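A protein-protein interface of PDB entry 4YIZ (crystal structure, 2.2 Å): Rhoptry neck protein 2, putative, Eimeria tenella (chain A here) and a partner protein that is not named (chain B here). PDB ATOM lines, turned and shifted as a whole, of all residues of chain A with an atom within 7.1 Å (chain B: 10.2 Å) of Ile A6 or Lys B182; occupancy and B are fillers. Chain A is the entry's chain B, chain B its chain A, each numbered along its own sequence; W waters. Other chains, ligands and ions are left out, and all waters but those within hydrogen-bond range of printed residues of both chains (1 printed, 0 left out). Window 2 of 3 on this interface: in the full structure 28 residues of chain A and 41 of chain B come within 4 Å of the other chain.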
ATOM      1  N   SER A   2     -15.579  11.307  -8.302  1.00  0.00           N
ATOM      2  CA  SER A   2     -14.672  10.267  -7.831  1.00  0.00           C
ATOM      3  C   SER A   2     -14.224  10.532  -6.395  1.00  0.00           C
ATOM      4  O   SER A   2     -13.725   9.632  -5.718  1.00  0.00           O
ATOM      5  CB  SER A   2     -13.457  10.164  -8.755  1.00  0.00           C
ATOM      6  OG  SER A   2     -13.836   9.706 -10.042  1.00  0.00           O
ATOM      7  N   ALA A   3     -14.402  11.771  -5.942  1.00  0.00           N
ATOM      8  CA  ALA A   3     -14.154  12.136  -4.550  1.00  0.00           C
ATOM      9  C   ALA A   3     -15.471  12.530  -3.888  1.00  0.00           C
ATOM     10  O   ALA A   3     -15.656  12.347  -2.684  1.00  0.00           O
ATOM     11  CB  ALA A   3     -13.144  13.266  -4.464  1.00  0.00           C
ATOM     12  N   SER A   4     -16.382  13.073  -4.689  1.00  0.00           N
ATOM     13  CA  SER A   4     -17.746  13.336  -4.247  1.00  0.00           C
ATOM     14  C   SER A   4     -18.486  12.013  -4.094  1.00  0.00           C
ATOM     15  O   SER A   4     -19.323  11.859  -3.208  1.00  0.00           O
ATOM     16  CB  SER A   4     -18.463  14.257  -5.241  1.00  0.00           C
ATOM     17  OG  SER A   4     -19.873  14.164  -5.137  1.00  0.00           O
ATOM     18  N   ASP A   5     -18.158  11.057  -4.960  1.00  0.00           N
ATOM     19  CA  ASP A   5     -18.744   9.722  -4.909  1.00  0.00           C
ATOM     20  C   ASP A   5     -18.378   9.019  -3.607  1.00  0.00           C
ATOM     21  O   ASP A   5     -19.224   8.384  -2.981  1.00  0.00           O
ATOM     22  CB  ASP A   5     -18.282   8.889  -6.110  1.00  0.00           C
ATOM     23  CG  ASP A   5     -19.171   9.072  -7.327  1.00  0.00           C
ATOM     24  OD1 ASP A   5     -19.854  10.115  -7.418  1.00  0.00           O
ATOM     25  OD2 ASP A   5     -19.184   8.173  -8.195  1.00  0.00           O
ATOM     26  N   ILE A   6     -17.117   9.141  -3.206  1.00  0.00           N
ATOM     27  CA  ILE A   6     -16.637   8.560  -1.956  1.00  0.00           C
ATOM     28  C   ILE A   6     -17.368   9.186  -0.772  1.00  0.00           C
ATOM     29  O   ILE A   6     -17.804   8.488   0.143  1.00  0.00           O
ATOM     30  CB  ILE A   6     -15.105   8.748  -1.815  1.00  0.00           C
ATOM     31  CG1 ILE A   6     -14.378   7.625  -2.558  1.00  0.00           C
ATOM     32  CG2 ILE A   6     -14.663   8.757  -0.347  1.00  0.00           C
ATOM     33  CD1 ILE A   6     -12.904   7.887  -2.810  1.00  0.00           C
ATOM     34  N   THR A   7     -17.501  10.508  -0.803  1.00  0.00           N
ATOM     35  CA  THR A   7     -18.253  11.242   0.208  1.00  0.00           C
ATOM     36  C   THR A   7     -19.687  10.733   0.275  1.00  0.00           C
ATOM     37  O   THR A   7     -20.209  10.432   1.354  1.00  0.00           O
ATOM     38  CB  THR A   7     -18.235  12.764  -0.093  1.00  0.00           C
ATOM     39  OG1 THR A   7     -17.066  13.349   0.490  1.00  0.00           O
ATOM     40  CG2 THR A   7     -19.474  13.480   0.453  1.00  0.00           C
ATOM     41  N   GLN A   8     -20.314  10.629  -0.891  1.00  0.00           N
ATOM     42  CA  GLN A   8     -21.678  10.131  -0.983  1.00  0.00           C
ATOM     43  C   GLN A   8     -21.759   8.715  -0.422  1.00  0.00           C
ATOM     44  O   GLN A   8     -22.703   8.382   0.288  1.00  0.00           O
ATOM     45  CB  GLN A   8     -22.176  10.159  -2.433  1.00  0.00           C
ATOM     46  CG  GLN A   8     -23.678   9.939  -2.570  1.00  0.00           C
ATOM     47  CD  GLN A   8     -24.485  10.929  -1.746  1.00  0.00           C
ATOM     48  OE1 GLN A   8     -24.100  12.090  -1.602  1.00  0.00           O
ATOM     49  NE2 GLN A   8     -25.598  10.470  -1.186  1.00  0.00           N
ATOM     50  N   HIS A   9     -20.762   7.889  -0.735  1.00  0.00           N
ATOM     51  CA  HIS A   9     -20.693   6.530  -0.206  1.00  0.00           C
ATOM     52  C   HIS A   9     -20.606   6.559   1.316  1.00  0.00           C
ATOM     53  O   HIS A   9     -21.282   5.785   1.994  1.00  0.00           O
ATOM     54  CB  HIS A   9     -19.491   5.768  -0.777  1.00  0.00           C
ATOM     55  CG  HIS A   9     -19.381   4.361  -0.276  1.00  0.00           C
ATOM     56  ND1 HIS A   9     -20.308   3.388  -0.584  1.00  0.00           N
ATOM     57  CD2 HIS A   9     -18.464   3.767   0.523  1.00  0.00           C
ATOM     58  CE1 HIS A   9     -19.961   2.253  -0.003  1.00  0.00           C
ATOM     59  NE2 HIS A   9     -18.845   2.456   0.675  1.00  0.00           N
ATOM     60  N   LEU A  10     -19.768   7.444   1.847  1.00  0.00           N
ATOM     61  CA  LEU A  10     -19.657   7.607   3.293  1.00  0.00           C
ATOM     62  C   LEU A  10     -20.993   7.997   3.907  1.00  0.00           C
ATOM     63  O   LEU A  10     -21.410   7.410   4.907  1.00  0.00           O
ATOM     64  CB  LEU A  10     -18.596   8.654   3.648  1.00  0.00           C
ATOM     65  CG  LEU A  10     -17.139   8.226   3.448  1.00  0.00           C
ATOM     66  CD1 LEU A  10     -16.209   9.412   3.645  1.00  0.00           C
ATOM     67  CD2 LEU A  10     -16.766   7.095   4.396  1.00  0.00           C
ATOM     68  N   ASN A  11     -21.664   8.983   3.321  1.00  0.00           N
ATOM     69  CA  ASN A  11     -22.986   9.361   3.811  1.00  0.00           C
ATOM     70  C   ASN A  11     -23.993   8.215   3.714  1.00  0.00           C
ATOM     71  O   ASN A  11     -24.797   8.011   4.621  1.00  0.00           O
ATOM     72  CB  ASN A  11     -23.518  10.576   3.046  1.00  0.00           C
ATOM     73  CG  ASN A  11     -24.896  11.000   3.524  1.00  0.00           C
ATOM     74  OD1 ASN A  11     -25.914  10.572   2.977  1.00  0.00           O
ATOM     75  ND2 ASN A  11     -24.936  11.831   4.559  1.00  0.00           N
ATOM     76  N   ASP A  12     -23.945   7.468   2.614  1.00  0.00           N
ATOM     77  CA  ASP A  12     -24.837   6.328   2.419  1.00  0.00           C
ATOM     78  C   ASP A  12     -24.550   5.202   3.409  1.00  0.00           C
ATOM     79  O   ASP A  12     -25.434   4.409   3.729  1.00  0.00           O
ATOM     80  CB  ASP A  12     -24.719   5.800   0.984  1.00  0.00           C
ATOM     81  CG  ASP A  12     -25.243   6.785  -0.046  1.00  0.00           C
ATOM     82  OD1 ASP A  12     -26.052   7.665   0.323  1.00  0.00           O
ATOM     83  OD2 ASP A  12     -24.850   6.679  -1.227  1.00  0.00           O
ATOM     84  N   SER A  13     -23.313   5.140   3.893  1.00  0.00           N
ATOM     85  CA  SER A  13     -22.899   4.093   4.825  1.00  0.00           C
ATOM     86  C   SER A  13     -23.192   4.460   6.281  1.00  0.00           C
ATOM     87  O   SER A  13     -22.948   3.660   7.185  1.00  0.00           O
ATOM     88  CB  SER A  13     -21.408   3.801   4.657  1.00  0.00           C
ATOM     89  OG  SER A  13     -21.136   3.257   3.376  1.00  0.00           O
ATOM     90  N   MET B 175     -21.812   4.055  11.491  1.00  0.00           N
ATOM     91  CA  MET B 175     -21.453   3.169  10.390  1.00  0.00           C
ATOM     92  C   MET B 175     -21.195   1.774  10.944  1.00  0.00           C
ATOM     93  O   MET B 175     -20.752   1.629  12.082  1.00  0.00           O
ATOM     94  CB  MET B 175     -20.217   3.683   9.646  1.00  0.00           C
ATOM     95  CG  MET B 175     -20.404   5.023   8.962  1.00  0.00           C
ATOM     96  SD  MET B 175     -19.033   5.409   7.856  1.00  0.00           S
ATOM     97  CE  MET B 175     -17.698   5.669   9.023  1.00  0.00           C
ATOM     98  N   MET B 178     -17.750  -1.059   6.156  1.00  0.00           N
ATOM     99  CA  MET B 178     -17.007  -0.367   5.111  1.00  0.00           C
ATOM    100  C   MET B 178     -15.965  -1.306   4.515  1.00  0.00           C
ATOM    101  O   MET B 178     -15.156  -1.891   5.240  1.00  0.00           O
ATOM    102  CB  MET B 178     -16.335   0.896   5.646  1.00  0.00           C
ATOM    103  CG  MET B 178     -16.102   1.942   4.564  1.00  0.00           C
ATOM    104  SD  MET B 178     -14.946   3.238   5.039  1.00  0.00           S
ATOM    105  CE  MET B 178     -15.981   4.267   6.075  1.00  0.00           C
ATOM    106  N   GLU B 179     -15.990  -1.438   3.192  1.00  0.00           N
ATOM    107  CA  GLU B 179     -15.147  -2.396   2.484  1.00  0.00           C
ATOM    108  C   GLU B 179     -14.723  -1.855   1.121  1.00  0.00           C
ATOM    109  O   GLU B 179     -15.346  -0.935   0.593  1.00  0.00           O
ATOM    110  CB  GLU B 179     -15.892  -3.720   2.309  1.00  0.00           C
ATOM    111  CG  GLU B 179     -17.173  -3.588   1.486  1.00  0.00           C
ATOM    112  CD  GLU B 179     -18.016  -4.848   1.494  1.00  0.00           C
ATOM    113  OE1 GLU B 179     -19.190  -4.781   1.071  1.00  0.00           O
ATOM    114  OE2 GLU B 179     -17.506  -5.907   1.922  1.00  0.00           O
ATOM    115  N   GLY B 180     -13.667  -2.437   0.558  1.00  0.00           N
ATOM    116  CA  GLY B 180     -13.177  -2.043  -0.752  1.00  0.00           C
ATOM    117  C   GLY B 180     -11.979  -1.119  -0.663  1.00  0.00           C
ATOM    118  O   GLY B 180     -12.021  -0.105   0.033  1.00  0.00           O
ATOM    119  N   LYS B 181     -10.913  -1.468  -1.381  1.00  0.00           N
ATOM    120  CA  LYS B 181      -9.675  -0.689  -1.377  1.00  0.00           C
ATOM    121  C   LYS B 181      -9.909   0.749  -1.837  1.00  0.00           C
ATOM    122  O   LYS B 181      -9.071   1.621  -1.632  1.00  0.00           O
ATOM    123  CB  LYS B 181      -8.625  -1.351  -2.275  1.00  0.00           C
ATOM    124  CG  LYS B 181      -8.864  -1.155  -3.769  1.00  0.00           C
ATOM    125  CD  LYS B 181      -7.835  -1.896  -4.607  1.00  0.00           C
ATOM    126  CE  LYS B 181      -8.148  -1.787  -6.090  1.00  0.00           C
ATOM    127  NZ  LYS B 181      -8.339  -3.124  -6.716  1.00  0.00           N
ATOM    128  N   LYS B 182     -11.050   0.983  -2.470  1.00  0.00           N
ATOM    129  CA  LYS B 182     -11.421   2.311  -2.932  1.00  0.00           C
ATOM    130  C   LYS B 182     -11.804   3.227  -1.768  1.00  0.00           C
ATOM    131  O   LYS B 182     -11.741   4.452  -1.886  1.00  0.00           O
ATOM    132  CB  LYS B 182     -12.581   2.196  -3.923  1.00  0.00           C
ATOM    133  CG  LYS B 182     -12.909   3.459  -4.692  1.00  0.00           C
ATOM    134  CD  LYS B 182     -13.745   3.127  -5.923  1.00  0.00           C
ATOM    135  CE  LYS B 182     -14.866   4.128  -6.142  1.00  0.00           C
ATOM    136  NZ  LYS B 182     -14.363   5.513  -6.349  1.00  0.00           N
ATOM    137  N   TYR B 183     -12.185   2.621  -0.644  1.00  0.00           N
ATOM    138  CA  TYR B 183     -12.778   3.353   0.473  1.00  0.00           C
ATOM    139  C   TYR B 183     -11.989   3.235   1.774  1.00  0.00           C
ATOM    140  O   TYR B 183     -12.023   4.141   2.603  1.00  0.00           O
ATOM    141  CB  TYR B 183     -14.206   2.860   0.711  1.00  0.00           C
ATOM    142  CG  TYR B 183     -15.123   3.066  -0.472  1.00  0.00           C
ATOM    143  CD1 TYR B 183     -15.525   4.340  -0.843  1.00  0.00           C
ATOM    144  CD2 TYR B 183     -15.590   1.988  -1.211  1.00  0.00           C
ATOM    145  CE1 TYR B 183     -16.363   4.539  -1.922  1.00  0.00           C
ATOM    146  CE2 TYR B 183     -16.430   2.176  -2.292  1.00  0.00           C
ATOM    147  CZ  TYR B 183     -16.814   3.454  -2.642  1.00  0.00           C
ATOM    148  OH  TYR B 183     -17.651   3.655  -3.715  1.00  0.00           O
ATOM    149  N   CYS B 184     -11.291   2.119   1.960  1.00  0.00           N
ATOM    150  CA  CYS B 184     -10.626   1.860   3.230  1.00  0.00           C
ATOM    151  C   CYS B 184      -9.479   0.866   3.103  1.00  0.00           C
ATOM    152  O   CYS B 184      -9.369   0.145   2.110  1.00  0.00           O
ATOM    153  CB  CYS B 184     -11.642   1.347   4.255  1.00  0.00           C
ATOM    154  SG  CYS B 184     -12.523  -0.150   3.738  1.00  0.00           S
ATOM    155  N   SER B 185      -8.637   0.834   4.131  1.00  0.00           N
ATOM    156  CA  SER B 185      -7.441   0.001   4.142  1.00  0.00           C
ATOM    157  C   SER B 185      -7.593  -1.207   5.055  1.00  0.00           C
ATOM    158  O   SER B 185      -8.360  -1.181   6.019  1.00  0.00           O
ATOM    159  CB  SER B 185      -6.231   0.824   4.591  1.00  0.00           C
ATOM    160  OG  SER B 185      -6.449   1.375   5.879  1.00  0.00           O
ATOM    161  N   VAL B 186      -6.842  -2.255   4.735  1.00  0.00           N
ATOM    162  CA  VAL B 186      -6.763  -3.460   5.549  1.00  0.00           C
ATOM    163  C   VAL B 186      -5.351  -3.577   6.108  1.00  0.00           C
ATOM    164  O   VAL B 186      -4.392  -3.747   5.354  1.00  0.00           O
ATOM    165  CB  VAL B 186      -7.112  -4.722   4.730  1.00  0.00           C
ATOM    166  CG1 VAL B 186      -6.923  -5.980   5.560  1.00  0.00           C
ATOM    167  CG2 VAL B 186      -8.535  -4.639   4.218  1.00  0.00           C
ATOM    168  N   GLU B 189      -3.013  -1.040   4.529  1.00  0.00           N
ATOM    169  CA  GLU B 189      -2.823  -1.087   3.079  1.00  0.00           C
ATOM    170  C   GLU B 189      -4.143  -0.869   2.339  1.00  0.00           C
ATOM    171  O   GLU B 189      -5.099  -1.614   2.560  1.00  0.00           O
ATOM    172  CB  GLU B 189      -2.214  -2.426   2.661  1.00  0.00           C
ATOM    173  CG  GLU B 189      -0.779  -2.632   3.132  1.00  0.00           C
ATOM    174  CD  GLU B 189       0.199  -1.661   2.491  1.00  0.00           C
ATOM    175  OE1 GLU B 189       0.002  -1.300   1.311  1.00  0.00           O
ATOM    176  OE2 GLU B 189       1.164  -1.256   3.172  1.00  0.00           O
ATOM    177  N   PRO B 190      -4.211   0.145   1.454  1.00  0.00           N
ATOM    178  CA  PRO B 190      -3.190   1.143   1.103  1.00  0.00           C
ATOM    179  C   PRO B 190      -3.085   2.267   2.139  1.00  0.00           C
ATOM    180  O   PRO B 190      -4.088   2.610   2.763  1.00  0.00           O
ATOM    181  CB  PRO B 190      -3.680   1.681  -0.243  1.00  0.00           C
ATOM    182  CG  PRO B 190      -5.147   1.523  -0.195  1.00  0.00           C
ATOM    183  CD  PRO B 190      -5.409   0.275   0.603  1.00  0.00           C
ATOM    184  N   ASP B 192      -2.729   5.482   1.931  1.00  0.00           N
ATOM    185  CA  ASP B 192      -3.237   6.811   1.591  1.00  0.00           C
ATOM    186  C   ASP B 192      -4.625   7.082   2.177  1.00  0.00           C
ATOM    187  O   ASP B 192      -5.084   8.224   2.197  1.00  0.00           O
ATOM    188  CB  ASP B 192      -3.293   6.988   0.068  1.00  0.00           C
ATOM    189  CG  ASP B 192      -1.928   6.854  -0.591  1.00  0.00           C
ATOM    190  OD1 ASP B 192      -0.918   7.242   0.031  1.00  0.00           O
ATOM    191  OD2 ASP B 192      -1.866   6.364  -1.740  1.00  0.00           O
ATOM    192  N   LEU B 193      -5.288   6.034   2.655  1.00  0.00           N
ATOM    193  CA  LEU B 193      -6.688   6.139   3.054  1.00  0.00           C
ATOM    194  C   LEU B 193      -6.879   6.465   4.532  1.00  0.00           C
ATOM    195  O   LEU B 193      -6.149   5.981   5.397  1.00  0.00           O
ATOM    196  CB  LEU B 193      -7.418   4.840   2.720  1.00  0.00           C
ATOM    197  CG  LEU B 193      -7.458   4.496   1.230  1.00  0.00           C
ATOM    198  CD1 LEU B 193      -8.006   3.103   1.040  1.00  0.00           C
ATOM    199  CD2 LEU B 193      -8.293   5.505   0.450  1.00  0.00           C
ATOM    200  N   THR B 194      -7.885   7.289   4.800  1.00  0.00           N
ATOM    201  CA  THR B 194      -8.233   7.695   6.153  1.00  0.00           C
ATOM    202  C   THR B 194      -8.818   6.539   6.955  1.00  0.00           C
ATOM    203  O   THR B 194      -8.429   6.303   8.099  1.00  0.00           O
ATOM    204  CB  THR B 194      -9.252   8.850   6.127  1.00  0.00           C
ATOM    205  OG1 THR B 194      -8.665   9.993   5.496  1.00  0.00           O
ATOM    206  CG2 THR B 194      -9.701   9.227   7.535  1.00  0.00           C
ATOM    207  N   TRP B 195      -9.759   5.826   6.346  1.00  0.00           N
ATOM    208  CA  TRP B 195     -10.522   4.806   7.056  1.00  0.00           C
ATOM    209  C   TRP B 195      -9.919   3.414   6.959  1.00  0.00           C
ATOM    210  O   TRP B 195      -9.468   2.981   5.901  1.00  0.00           O
ATOM    211  CB  TRP B 195     -11.959   4.766   6.533  1.00  0.00           C
ATOM    212  CG  TRP B 195     -12.829   5.822   7.128  1.00  0.00           C
ATOM    213  CD1 TRP B 195     -13.254   6.972   6.527  1.00  0.00           C
ATOM    214  CD2 TRP B 195     -13.384   5.831   8.448  1.00  0.00           C
ATOM    215  NE1 TRP B 195     -14.040   7.695   7.392  1.00  0.00           N
ATOM    216  CE2 TRP B 195     -14.134   7.016   8.579  1.00  0.00           C
ATOM    217  CE3 TRP B 195     -13.317   4.950   9.534  1.00  0.00           C
ATOM    218  CZ2 TRP B 195     -14.813   7.344   9.751  1.00  0.00           C
ATOM    219  CZ3 TRP B 195     -13.993   5.279  10.696  1.00  0.00           C
ATOM    220  CH2 TRP B 195     -14.732   6.465  10.795  1.00  0.00           C
ATOM    221  N   TYR B 196      -9.898   2.736   8.099  1.00  0.00           N
ATOM    222  CA  TYR B 196      -9.680   1.300   8.155  1.00  0.00           C
ATOM    223  C   TYR B 196     -10.982   0.624   7.753  1.00  0.00           C
ATOM    224  O   TYR B 196     -12.059   1.198   7.925  1.00  0.00           O
ATOM    225  CB  TYR B 196      -9.258   0.860   9.559  1.00  0.00           C
ATOM    226  CG  TYR B 196     -10.127   1.456  10.645  1.00  0.00           C
ATOM    227  CD1 TYR B 196     -11.352   0.891  10.977  1.00  0.00           C
ATOM    228  CD2 TYR B 196      -9.734   2.601  11.319  1.00  0.00           C
ATOM    229  CE1 TYR B 196     -12.151   1.446  11.958  1.00  0.00           C
ATOM    230  CE2 TYR B 196     -10.523   3.162  12.299  1.00  0.00           C
ATOM    231  CZ  TYR B 196     -11.730   2.581  12.615  1.00  0.00           C
ATOM    232  OH  TYR B 196     -12.514   3.144  13.592  1.00  0.00           O
ATOM    233  N   CYS B 197     -10.894  -0.584   7.209  1.00  0.00           N
ATOM    234  CA  CYS B 197     -12.090  -1.349   6.888  1.00  0.00           C
ATOM    235  C   CYS B 197     -12.653  -1.986   8.152  1.00  0.00           C
ATOM    236  O   CYS B 197     -11.923  -2.244   9.107  1.00  0.00           O
ATOM    237  CB  CYS B 197     -11.782  -2.416   5.837  1.00  0.00           C
ATOM    238  SG  CYS B 197     -11.322  -1.719   4.224  1.00  0.00           S
ATOM    239  N   PRO B 281     -25.692   0.218   1.560  1.00  0.00           N
ATOM    240  CA  PRO B 281     -25.827   0.523   0.129  1.00  0.00           C
ATOM    241  C   PRO B 281     -25.330  -0.605  -0.767  1.00  0.00           C
ATOM    242  O   PRO B 281     -24.351  -1.252  -0.396  1.00  0.00           O
ATOM    243  CB  PRO B 281     -24.959   1.776  -0.051  1.00  0.00           C
ATOM    244  CG  PRO B 281     -24.071   1.819   1.149  1.00  0.00           C
ATOM    245  CD  PRO B 281     -24.889   1.241   2.251  1.00  0.00           C
HETATM  246  O   HOH W   1     -18.043  -0.027   1.837  1.00  0.00           O
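The side-chain sulfur of Cys B197 forms a disulfide with the side-chain sulfur of Cys B184 (2.0 Å). The side-chain amide nitrogen (NE2) of Gln A8 sits at hydrogen-bond distance from the side-chain carboxylate (OD1) of Asp A12 (3.2 Å). The backbone carbonyl oxygen (O) of His A9 sits at hydrogen-bond distance from the side-chain hydroxyl (OG) of Ser A13 (2.9 Å).
Lys B182 touches Ile A6 (O to CD1, 3.7 Å). Ile A6 touches Tyr B183 (CG1 to CE1, 3.7 Å). Tyr B183 touches His A9 (CD1 to CD2, 3.3 Å). Leu A10 touches Met B178. Asp A12 touches Pro B281. CG of Met B175 touches O of Ser A13, 3.4 Å away. Pro B281 touches Ser A13.
No residue of chain B comes within 4 Å of Ala A3. No residue of chain B comes within 4 Å of Asp A5. Ile A6 touches two residues of chain B. No residue of chain B comes within 4 Å of Thr A7. Of chain B, only Met B178 (3.4 Å) comes within 4 Å of Leu A10. Printed residues of chain B within 4 Å of Asp A12: Pro B281. Lys B181 touches none of the printed residues of chain A. Lys B182 touches just one residue of chain A: Ile A6. Of the printed residues of chain A, Tyr B183 touches Ile A6 (3.7 Å) and His A9 (3.3 Å). Cys B197 touches none of the printed residues of chain A. Printed residues of chain A within 4 Å of Pro B281: Asp A12 and Ser A13.
Hydrophobic or aromatic side chains of chain A that line the printed part of chain B: Ile A6, His A9 and Leu A10. Hydrophobic or aromatic side chains of chain B within 4 Å of the printed part of chain A: Met B175, Met B178, Tyr B183 and Pro B281.
Water W1 lies within hydrogen-bond range of N of Glu B179 (2.8 Å) and NE2 of His A9 (2.9 Å).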
